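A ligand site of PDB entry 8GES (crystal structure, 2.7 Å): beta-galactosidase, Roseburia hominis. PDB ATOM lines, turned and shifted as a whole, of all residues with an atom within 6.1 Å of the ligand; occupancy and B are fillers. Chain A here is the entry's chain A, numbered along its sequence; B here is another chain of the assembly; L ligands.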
ATOM      1  N   ASP A 156     -27.098  33.164 -31.505  1.00  0.00           N
ATOM      2  CA  ASP A 156     -27.267  31.760 -31.158  1.00  0.00           C
ATOM      3  C   ASP A 156     -28.138  31.588 -29.923  1.00  0.00           C
ATOM      4  O   ASP A 156     -27.883  32.215 -28.884  1.00  0.00           O
ATOM      5  CB  ASP A 156     -25.905  31.100 -30.943  1.00  0.00           C
ATOM      6  CG  ASP A 156     -25.935  29.612 -31.196  1.00  0.00           C
ATOM      7  OD1 ASP A 156     -27.019  29.005 -31.056  1.00  0.00           O
ATOM      8  OD2 ASP A 156     -24.874  29.035 -31.531  1.00  0.00           O
ATOM      9  N   TYR A 159     -26.960  26.925 -28.290  1.00  0.00           N
ATOM     10  CA  TYR A 159     -25.689  26.410 -27.797  1.00  0.00           C
ATOM     11  C   TYR A 159     -25.699  26.413 -26.271  1.00  0.00           C
ATOM     12  O   TYR A 159     -25.234  27.351 -25.616  1.00  0.00           O
ATOM     13  CB  TYR A 159     -24.500  27.211 -28.322  1.00  0.00           C
ATOM     14  CG  TYR A 159     -23.206  26.516 -27.965  1.00  0.00           C
ATOM     15  CD1 TYR A 159     -22.838  25.335 -28.601  1.00  0.00           C
ATOM     16  CD2 TYR A 159     -22.403  26.993 -26.941  1.00  0.00           C
ATOM     17  CE1 TYR A 159     -21.679  24.683 -28.261  1.00  0.00           C
ATOM     18  CE2 TYR A 159     -21.235  26.345 -26.600  1.00  0.00           C
ATOM     19  CZ  TYR A 159     -20.882  25.187 -27.261  1.00  0.00           C
ATOM     20  OH  TYR A 159     -19.714  24.539 -26.920  1.00  0.00           O
ATOM     21  N   TYR A 160     -26.230  25.327 -25.700  1.00  0.00           N
ATOM     22  CA  TYR A 160     -26.199  25.109 -24.257  1.00  0.00           C
ATOM     23  C   TYR A 160     -26.765  26.312 -23.493  1.00  0.00           C
ATOM     24  O   TYR A 160     -26.235  26.729 -22.464  1.00  0.00           O
ATOM     25  CB  TYR A 160     -24.772  24.787 -23.790  1.00  0.00           C
ATOM     26  CG  TYR A 160     -24.238  23.473 -24.318  1.00  0.00           C
ATOM     27  CD1 TYR A 160     -23.646  23.397 -25.573  1.00  0.00           C
ATOM     28  CD2 TYR A 160     -24.330  22.306 -23.572  1.00  0.00           C
ATOM     29  CE1 TYR A 160     -23.157  22.199 -26.059  1.00  0.00           C
ATOM     30  CE2 TYR A 160     -23.847  21.093 -24.052  1.00  0.00           C
ATOM     31  CZ  TYR A 160     -23.253  21.059 -25.295  1.00  0.00           C
ATOM     32  OH  TYR A 160     -22.764  19.861 -25.781  1.00  0.00           O
ATOM     33  N   GLY A 162     -26.741  29.433 -23.907  1.00  0.00           N
ATOM     34  CA  GLY A 162     -25.864  30.569 -23.707  1.00  0.00           C
ATOM     35  C   GLY A 162     -26.508  31.874 -24.120  1.00  0.00           C
ATOM     36  O   GLY A 162     -27.655  31.939 -24.580  1.00  0.00           O
ATOM     37  N   PRO A 163     -25.753  32.970 -23.942  1.00  0.00           N
ATOM     38  CA  PRO A 163     -26.246  34.293 -24.328  1.00  0.00           C
ATOM     39  C   PRO A 163     -25.934  34.690 -25.767  1.00  0.00           C
ATOM     40  O   PRO A 163     -26.440  35.729 -26.217  1.00  0.00           O
ATOM     41  CB  PRO A 163     -25.507  35.217 -23.354  1.00  0.00           C
ATOM     42  CG  PRO A 163     -24.201  34.528 -23.130  1.00  0.00           C
ATOM     43  CD  PRO A 163     -24.449  33.033 -23.265  1.00  0.00           C
ATOM     44  N   GLY A 164     -25.142  33.910 -26.494  1.00  0.00           N
ATOM     45  CA  GLY A 164     -24.788  34.270 -27.847  1.00  0.00           C
ATOM     46  C   GLY A 164     -23.761  35.373 -27.949  1.00  0.00           C
ATOM     47  O   GLY A 164     -23.575  35.936 -29.034  1.00  0.00           O
ATOM     48  N   ILE A 165     -23.080  35.683 -26.848  1.00  0.00           N
ATOM     49  CA  ILE A 165     -22.054  36.731 -26.831  1.00  0.00           C
ATOM     50  C   ILE A 165     -21.088  36.418 -25.705  1.00  0.00           C
ATOM     51  O   ILE A 165     -21.498  36.114 -24.580  1.00  0.00           O
ATOM     52  CB  ILE A 165     -22.675  38.131 -26.660  1.00  0.00           C
ATOM     53  CG1 ILE A 165     -21.594  39.201 -26.800  1.00  0.00           C
ATOM     54  CG2 ILE A 165     -23.386  38.246 -25.329  1.00  0.00           C
ATOM     55  CD1 ILE A 165     -22.150  40.599 -27.023  1.00  0.00           C
ATOM     56  N   LYS A 166     -19.788  36.498 -26.006  1.00  0.00           N
ATOM     57  CA  LYS A 166     -18.732  36.087 -25.080  1.00  0.00           C
ATOM     58  C   LYS A 166     -17.692  37.202 -24.990  1.00  0.00           C
ATOM     59  O   LYS A 166     -16.970  37.451 -25.963  1.00  0.00           O
ATOM     60  CB  LYS A 166     -18.100  34.765 -25.530  1.00  0.00           C
ATOM     61  CG  LYS A 166     -16.924  34.300 -24.706  1.00  0.00           C
ATOM     62  CD  LYS A 166     -16.141  33.223 -25.438  1.00  0.00           C
ATOM     63  CE  LYS A 166     -14.699  33.155 -24.968  1.00  0.00           C
ATOM     64  NZ  LYS A 166     -13.841  32.438 -25.945  1.00  0.00           N
ATOM     65  N   GLU A 181     -17.018  38.358 -28.729  1.00  0.00           N
ATOM     66  CA  GLU A 181     -17.350  37.261 -29.620  1.00  0.00           C
ATOM     67  C   GLU A 181     -18.844  36.996 -29.565  1.00  0.00           C
ATOM     68  O   GLU A 181     -19.415  36.833 -28.483  1.00  0.00           O
ATOM     69  CB  GLU A 181     -16.579  35.991 -29.250  1.00  0.00           C
ATOM     70  CG  GLU A 181     -16.442  34.997 -30.402  1.00  0.00           C
ATOM     71  CD  GLU A 181     -15.552  33.824 -30.058  1.00  0.00           C
ATOM     72  OE1 GLU A 181     -14.802  33.909 -29.059  1.00  0.00           O
ATOM     73  OE2 GLU A 181     -15.600  32.812 -30.778  1.00  0.00           O
ATOM     74  N   PHE A 183     -22.198  34.779 -31.650  1.00  0.00           N
ATOM     75  CA  PHE A 183     -22.470  33.542 -32.380  1.00  0.00           C
ATOM     76  C   PHE A 183     -23.848  33.637 -33.015  1.00  0.00           C
ATOM     77  O   PHE A 183     -24.819  34.035 -32.360  1.00  0.00           O
ATOM     78  CB  PHE A 183     -22.381  32.333 -31.456  1.00  0.00           C
ATOM     79  CG  PHE A 183     -21.140  32.312 -30.610  1.00  0.00           C
ATOM     80  CD1 PHE A 183     -21.114  32.951 -29.375  1.00  0.00           C
ATOM     81  CD2 PHE A 183     -19.992  31.678 -31.050  1.00  0.00           C
ATOM     82  CE1 PHE A 183     -19.972  32.938 -28.607  1.00  0.00           C
ATOM     83  CE2 PHE A 183     -18.845  31.657 -30.285  1.00  0.00           C
ATOM     84  CZ  PHE A 183     -18.838  32.289 -29.052  1.00  0.00           C
ATOM     85  N   LEU A 184     -23.937  33.249 -34.285  1.00  0.00           N
ATOM     86  CA  LEU A 184     -25.120  33.518 -35.106  1.00  0.00           C
ATOM     87  C   LEU A 184     -25.798  32.216 -35.528  1.00  0.00           C
ATOM     88  O   LEU A 184     -25.317  31.112 -35.266  1.00  0.00           O
ATOM     89  CB  LEU A 184     -24.753  34.348 -36.329  1.00  0.00           C
ATOM     90  CG  LEU A 184     -24.071  35.692 -36.019  1.00  0.00           C
ATOM     91  CD1 LEU A 184     -23.392  36.252 -37.258  1.00  0.00           C
ATOM     92  CD2 LEU A 184     -25.079  36.675 -35.456  1.00  0.00           C
ATOM     93  N   LYS A 359     -20.397  22.255 -18.854  1.00  0.00           N
ATOM     94  CA  LYS A 359     -20.395  23.061 -20.068  1.00  0.00           C
ATOM     95  C   LYS A 359     -21.451  24.154 -20.009  1.00  0.00           C
ATOM     96  O   LYS A 359     -21.217  25.282 -20.443  1.00  0.00           O
ATOM     97  CB  LYS A 359     -20.616  22.169 -21.288  1.00  0.00           C
ATOM     98  CG  LYS A 359     -19.358  21.861 -22.083  1.00  0.00           C
ATOM     99  CD  LYS A 359     -19.651  20.931 -23.246  1.00  0.00           C
ATOM    100  CE  LYS A 359     -19.831  21.710 -24.545  1.00  0.00           C
ATOM    101  NZ  LYS A 359     -19.511  20.880 -25.739  1.00  0.00           N
ATOM    102  N   VAL A 362     -20.360  27.112 -17.573  1.00  0.00           N
ATOM    103  CA  VAL A 362     -19.336  28.035 -18.074  1.00  0.00           C
ATOM    104  C   VAL A 362     -19.879  28.896 -19.207  1.00  0.00           C
ATOM    105  O   VAL A 362     -19.593  30.098 -19.270  1.00  0.00           O
ATOM    106  CB  VAL A 362     -18.090  27.242 -18.512  1.00  0.00           C
ATOM    107  CG1 VAL A 362     -17.151  28.135 -19.310  1.00  0.00           C
ATOM    108  CG2 VAL A 362     -17.374  26.665 -17.293  1.00  0.00           C
ATOM    109  N   VAL A 363     -20.673  28.311 -20.105  1.00  0.00           N
ATOM    110  CA  VAL A 363     -21.232  29.087 -21.201  1.00  0.00           C
ATOM    111  C   VAL A 363     -22.221  30.125 -20.683  1.00  0.00           C
ATOM    112  O   VAL A 363     -22.250  31.263 -21.144  1.00  0.00           O
ATOM    113  CB  VAL A 363     -21.891  28.161 -22.243  1.00  0.00           C
ATOM    114  CG1 VAL A 363     -22.785  28.956 -23.180  1.00  0.00           C
ATOM    115  CG2 VAL A 363     -20.830  27.397 -23.031  1.00  0.00           C
ATOM    116  N   GLN A 364     -23.042  29.738 -19.707  1.00  0.00           N
ATOM    117  CA  GLN A 364     -24.125  30.592 -19.218  1.00  0.00           C
ATOM    118  C   GLN A 364     -23.663  31.642 -18.217  1.00  0.00           C
ATOM    119  O   GLN A 364     -24.474  32.487 -17.816  1.00  0.00           O
ATOM    120  CB  GLN A 364     -25.224  29.737 -18.588  1.00  0.00           C
ATOM    121  CG  GLN A 364     -26.075  28.997 -19.599  1.00  0.00           C
ATOM    122  CD  GLN A 364     -27.046  28.037 -18.948  1.00  0.00           C
ATOM    123  OE1 GLN A 364     -27.557  28.284 -17.856  1.00  0.00           O
ATOM    124  NE2 GLN A 364     -27.314  26.923 -19.620  1.00  0.00           N
ATOM    125  N   TYR A 366     -19.932  32.758 -18.133  1.00  0.00           N
ATOM    126  CA  TYR A 366     -18.605  33.285 -18.447  1.00  0.00           C
ATOM    127  C   TYR A 366     -18.512  34.778 -18.188  1.00  0.00           C
ATOM    128  O   TYR A 366     -17.459  35.279 -17.766  1.00  0.00           O
ATOM    129  CB  TYR A 366     -18.280  32.968 -19.907  1.00  0.00           C
ATOM    130  CG  TYR A 366     -16.865  33.287 -20.350  1.00  0.00           C
ATOM    131  CD1 TYR A 366     -15.843  32.357 -20.186  1.00  0.00           C
ATOM    132  CD2 TYR A 366     -16.563  34.491 -20.955  1.00  0.00           C
ATOM    133  CE1 TYR A 366     -14.557  32.630 -20.598  1.00  0.00           C
ATOM    134  CE2 TYR A 366     -15.272  34.779 -21.373  1.00  0.00           C
ATOM    135  CZ  TYR A 366     -14.274  33.846 -21.191  1.00  0.00           C
ATOM    136  OH  TYR A 366     -12.988  34.118 -21.604  1.00  0.00           O
ATOM    137  N   GLU A 403      -9.939  24.702 -21.220  1.00  0.00           N
ATOM    138  CA  GLU A 403      -9.982  24.946 -22.656  1.00  0.00           C
ATOM    139  C   GLU A 403     -10.988  26.019 -23.038  1.00  0.00           C
ATOM    140  O   GLU A 403     -10.744  26.778 -23.988  1.00  0.00           O
ATOM    141  CB  GLU A 403     -10.289  23.639 -23.398  1.00  0.00           C
ATOM    142  CG  GLU A 403      -9.702  23.565 -24.800  1.00  0.00           C
ATOM    143  CD  GLU A 403     -10.435  24.430 -25.809  1.00  0.00           C
ATOM    144  OE1 GLU A 403     -11.576  24.069 -26.185  1.00  0.00           O
ATOM    145  OE2 GLU A 403      -9.880  25.465 -26.227  1.00  0.00           O
ATOM    146  N   MET A 404     -12.120  26.095 -22.344  1.00  0.00           N
ATOM    147  CA  MET A 404     -13.139  27.084 -22.647  1.00  0.00           C
ATOM    148  C   MET A 404     -12.908  28.417 -21.965  1.00  0.00           C
ATOM    149  O   MET A 404     -13.335  29.454 -22.484  1.00  0.00           O
ATOM    150  CB  MET A 404     -14.529  26.564 -22.252  1.00  0.00           C
ATOM    151  CG  MET A 404     -14.757  25.097 -22.545  1.00  0.00           C
ATOM    152  SD  MET A 404     -16.405  24.545 -22.052  1.00  0.00           S
ATOM    153  CE  MET A 404     -17.437  25.581 -23.074  1.00  0.00           C
ATOM    154  N   ASP A 405     -12.234  28.428 -20.817  1.00  0.00           N
ATOM    155  CA  ASP A 405     -12.102  29.647 -20.008  1.00  0.00           C
ATOM    156  C   ASP A 405     -10.657  29.764 -19.546  1.00  0.00           C
ATOM    157  O   ASP A 405     -10.237  29.058 -18.617  1.00  0.00           O
ATOM    158  CB  ASP A 405     -13.073  29.614 -18.833  1.00  0.00           C
ATOM    159  CG  ASP A 405     -12.995  30.867 -17.987  1.00  0.00           C
ATOM    160  OD1 ASP A 405     -12.297  31.819 -18.398  1.00  0.00           O
ATOM    161  OD2 ASP A 405     -13.634  30.902 -16.915  1.00  0.00           O
ATOM    162  N   GLU B  19     -20.477  11.691 -25.877  1.00  0.00           N
ATOM    163  CA  GLU B  19     -21.277  12.615 -26.665  1.00  0.00           C
ATOM    164  C   GLU B  19     -21.411  12.087 -28.085  1.00  0.00           C
ATOM    165  O   GLU B  19     -20.513  11.402 -28.599  1.00  0.00           O
ATOM    166  CB  GLU B  19     -20.653  14.019 -26.687  1.00  0.00           C
ATOM    167  CG  GLU B  19     -19.305  14.092 -27.394  1.00  0.00           C
ATOM    168  CD  GLU B  19     -18.817  15.516 -27.556  1.00  0.00           C
ATOM    169  OE1 GLU B  19     -18.604  16.194 -26.525  1.00  0.00           O
ATOM    170  OE2 GLU B  19     -18.652  15.973 -28.705  1.00  0.00           O
ATOM    171  N   LYS B  22     -19.768  14.215 -34.080  1.00  0.00           N
ATOM    172  CA  LYS B  22     -20.246  15.117 -35.123  1.00  0.00           C
ATOM    173  C   LYS B  22     -19.879  14.670 -36.525  1.00  0.00           C
ATOM    174  O   LYS B  22     -20.471  15.147 -37.492  1.00  0.00           O
ATOM    175  CB  LYS B  22     -19.701  16.526 -34.866  1.00  0.00           C
ATOM    176  CG  LYS B  22     -19.890  16.979 -33.429  1.00  0.00           C
ATOM    177  CD  LYS B  22     -18.859  18.016 -33.018  1.00  0.00           C
ATOM    178  CE  LYS B  22     -19.400  18.912 -31.904  1.00  0.00           C
ATOM    179  NZ  LYS B  22     -20.112  18.146 -30.843  1.00  0.00           N
HETATM  180  N1  LIG L   1     -20.257  28.701 -29.753  1.00  0.00           N
HETATM  181  C1  LIG L   1     -21.454  28.854 -30.421  1.00  0.00           C
HETATM  182  O1  LIG L   1     -21.588  28.436 -31.567  1.00  0.00           O
HETATM  183  N2  LIG L   1     -22.499  29.500 -29.803  1.00  0.00           N
HETATM  184  C2  LIG L   1     -22.351  29.980 -28.522  1.00  0.00           C
HETATM  185  O2  LIG L   1     -23.284  30.548 -27.971  1.00  0.00           O
HETATM  186  C3  LIG L   1     -21.141  29.819 -27.845  1.00  0.00           C
HETATM  187  N3  LIG L   1     -21.015  30.300 -26.565  1.00  0.00           N
HETATM  188  C4  LIG L   1     -19.831  30.150 -25.888  1.00  0.00           C
HETATM  189  C5  LIG L   1     -19.714  30.646 -24.594  1.00  0.00           C
HETATM  190  C6  LIG L   1     -18.527  30.502 -23.893  1.00  0.00           C
HETATM  191  C7  LIG L   1     -18.422  31.033 -22.496  1.00  0.00           C
HETATM  192  C8  LIG L   1     -17.453  29.850 -24.479  1.00  0.00           C
HETATM  193  C9  LIG L   1     -16.147  29.673 -23.749  1.00  0.00           C
HETATM  194  C10 LIG L   1     -17.578  29.371 -25.769  1.00  0.00           C
HETATM  195  C11 LIG L   1     -18.765  29.497 -26.485  1.00  0.00           C
HETATM  196  N4  LIG L   1     -18.873  29.004 -27.778  1.00  0.00           N
HETATM  197  C12 LIG L   1     -20.079  29.159 -28.466  1.00  0.00           C
HETATM  198  C13 LIG L   1     -17.662  28.314 -28.365  1.00  0.00           C
HETATM  199  C14 LIG L   1     -17.929  27.133 -29.298  1.00  0.00           C
HETATM  200  O3  LIG L   1     -19.165  26.549 -28.994  1.00  0.00           O
HETATM  201  C15 LIG L   1     -16.814  26.076 -29.175  1.00  0.00           C
HETATM  202  O4  LIG L   1     -15.552  26.714 -29.335  1.00  0.00           O
HETATM  203  C16 LIG L   1     -16.962  24.912 -30.135  1.00  0.00           C
HETATM  204  O5  LIG L   1     -17.954  25.255 -31.077  1.00  0.00           O
HETATM  205  C17 LIG L   1     -17.338  23.636 -29.389  1.00  0.00           C
HETATM  206  O6  LIG L   1     -18.468  23.034 -29.993  1.00  0.00           O
HETATM  207  P1  LIG L   1     -19.111  21.705 -29.344  1.00  0.00           P
HETATM  208  O7  LIG L   1     -19.349  21.970 -27.882  1.00  0.00           O
HETATM  209  O8  LIG L   1     -18.170  20.543 -29.516  1.00  0.00           O
HETATM  210  O9  LIG L   1     -20.439  21.401 -30.010  1.00  0.00           O
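An oxygen (O7) of the ligand lies within salt-bridge range of the side-chain amino group of Lys 359, at 2.4 Å.
O7 of the ligand lies within hydrogen-bond range of OH of Tyr 159 (2.8 Å).
N2 of the ligand sits at hydrogen-bond distance from OD2 of Asp 156, at 3.0 Å.
O8 of the ligand is in salt-bridge range of NZ of Lys 22 of chain B (3.4 Å).
Lys 166 touches the ligand.
CG of Phe 183 touches N2 of the ligand (3.2 Å).
Val 362 touches the ligand.
Val 363 touches the ligand.
CB of Tyr 366 touches C7 of the ligand, at 3.2 Å.
O of Met 404 touches C9 of the ligand, at 3.1 Å.
Hydrophobic or aromatic side chains within 4 Å of the ligand: Tyr 159, Phe 183, Val 363, Tyr 366 and Met 404.
The nearest printed residue that does not touch the ligand is Gly 164 (4.02 Å).
The side-chain amino group of Lys 359 is in hydrogen-bond range of the side-chain hydroxyl of Tyr 160, 3.4 Å away.
N of Tyr 159 is in hydrogen-bond range of OD1 of Asp 156 (3.5 Å).
The backbone NH of Asp 156 is in hydrogen-bond range of the backbone carbonyl oxygen of Phe 183.
NZ of Lys 22 of chain B is in salt-bridge range of OE2 of Glu 19 of chain B (3.4 Å).
N of Phe 183 sits at hydrogen-bond distance from O of Gly 164 (3.2 Å).
NZ of Lys 166 lies within salt-bridge range of OE1 of Glu 181 (3.6 Å).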
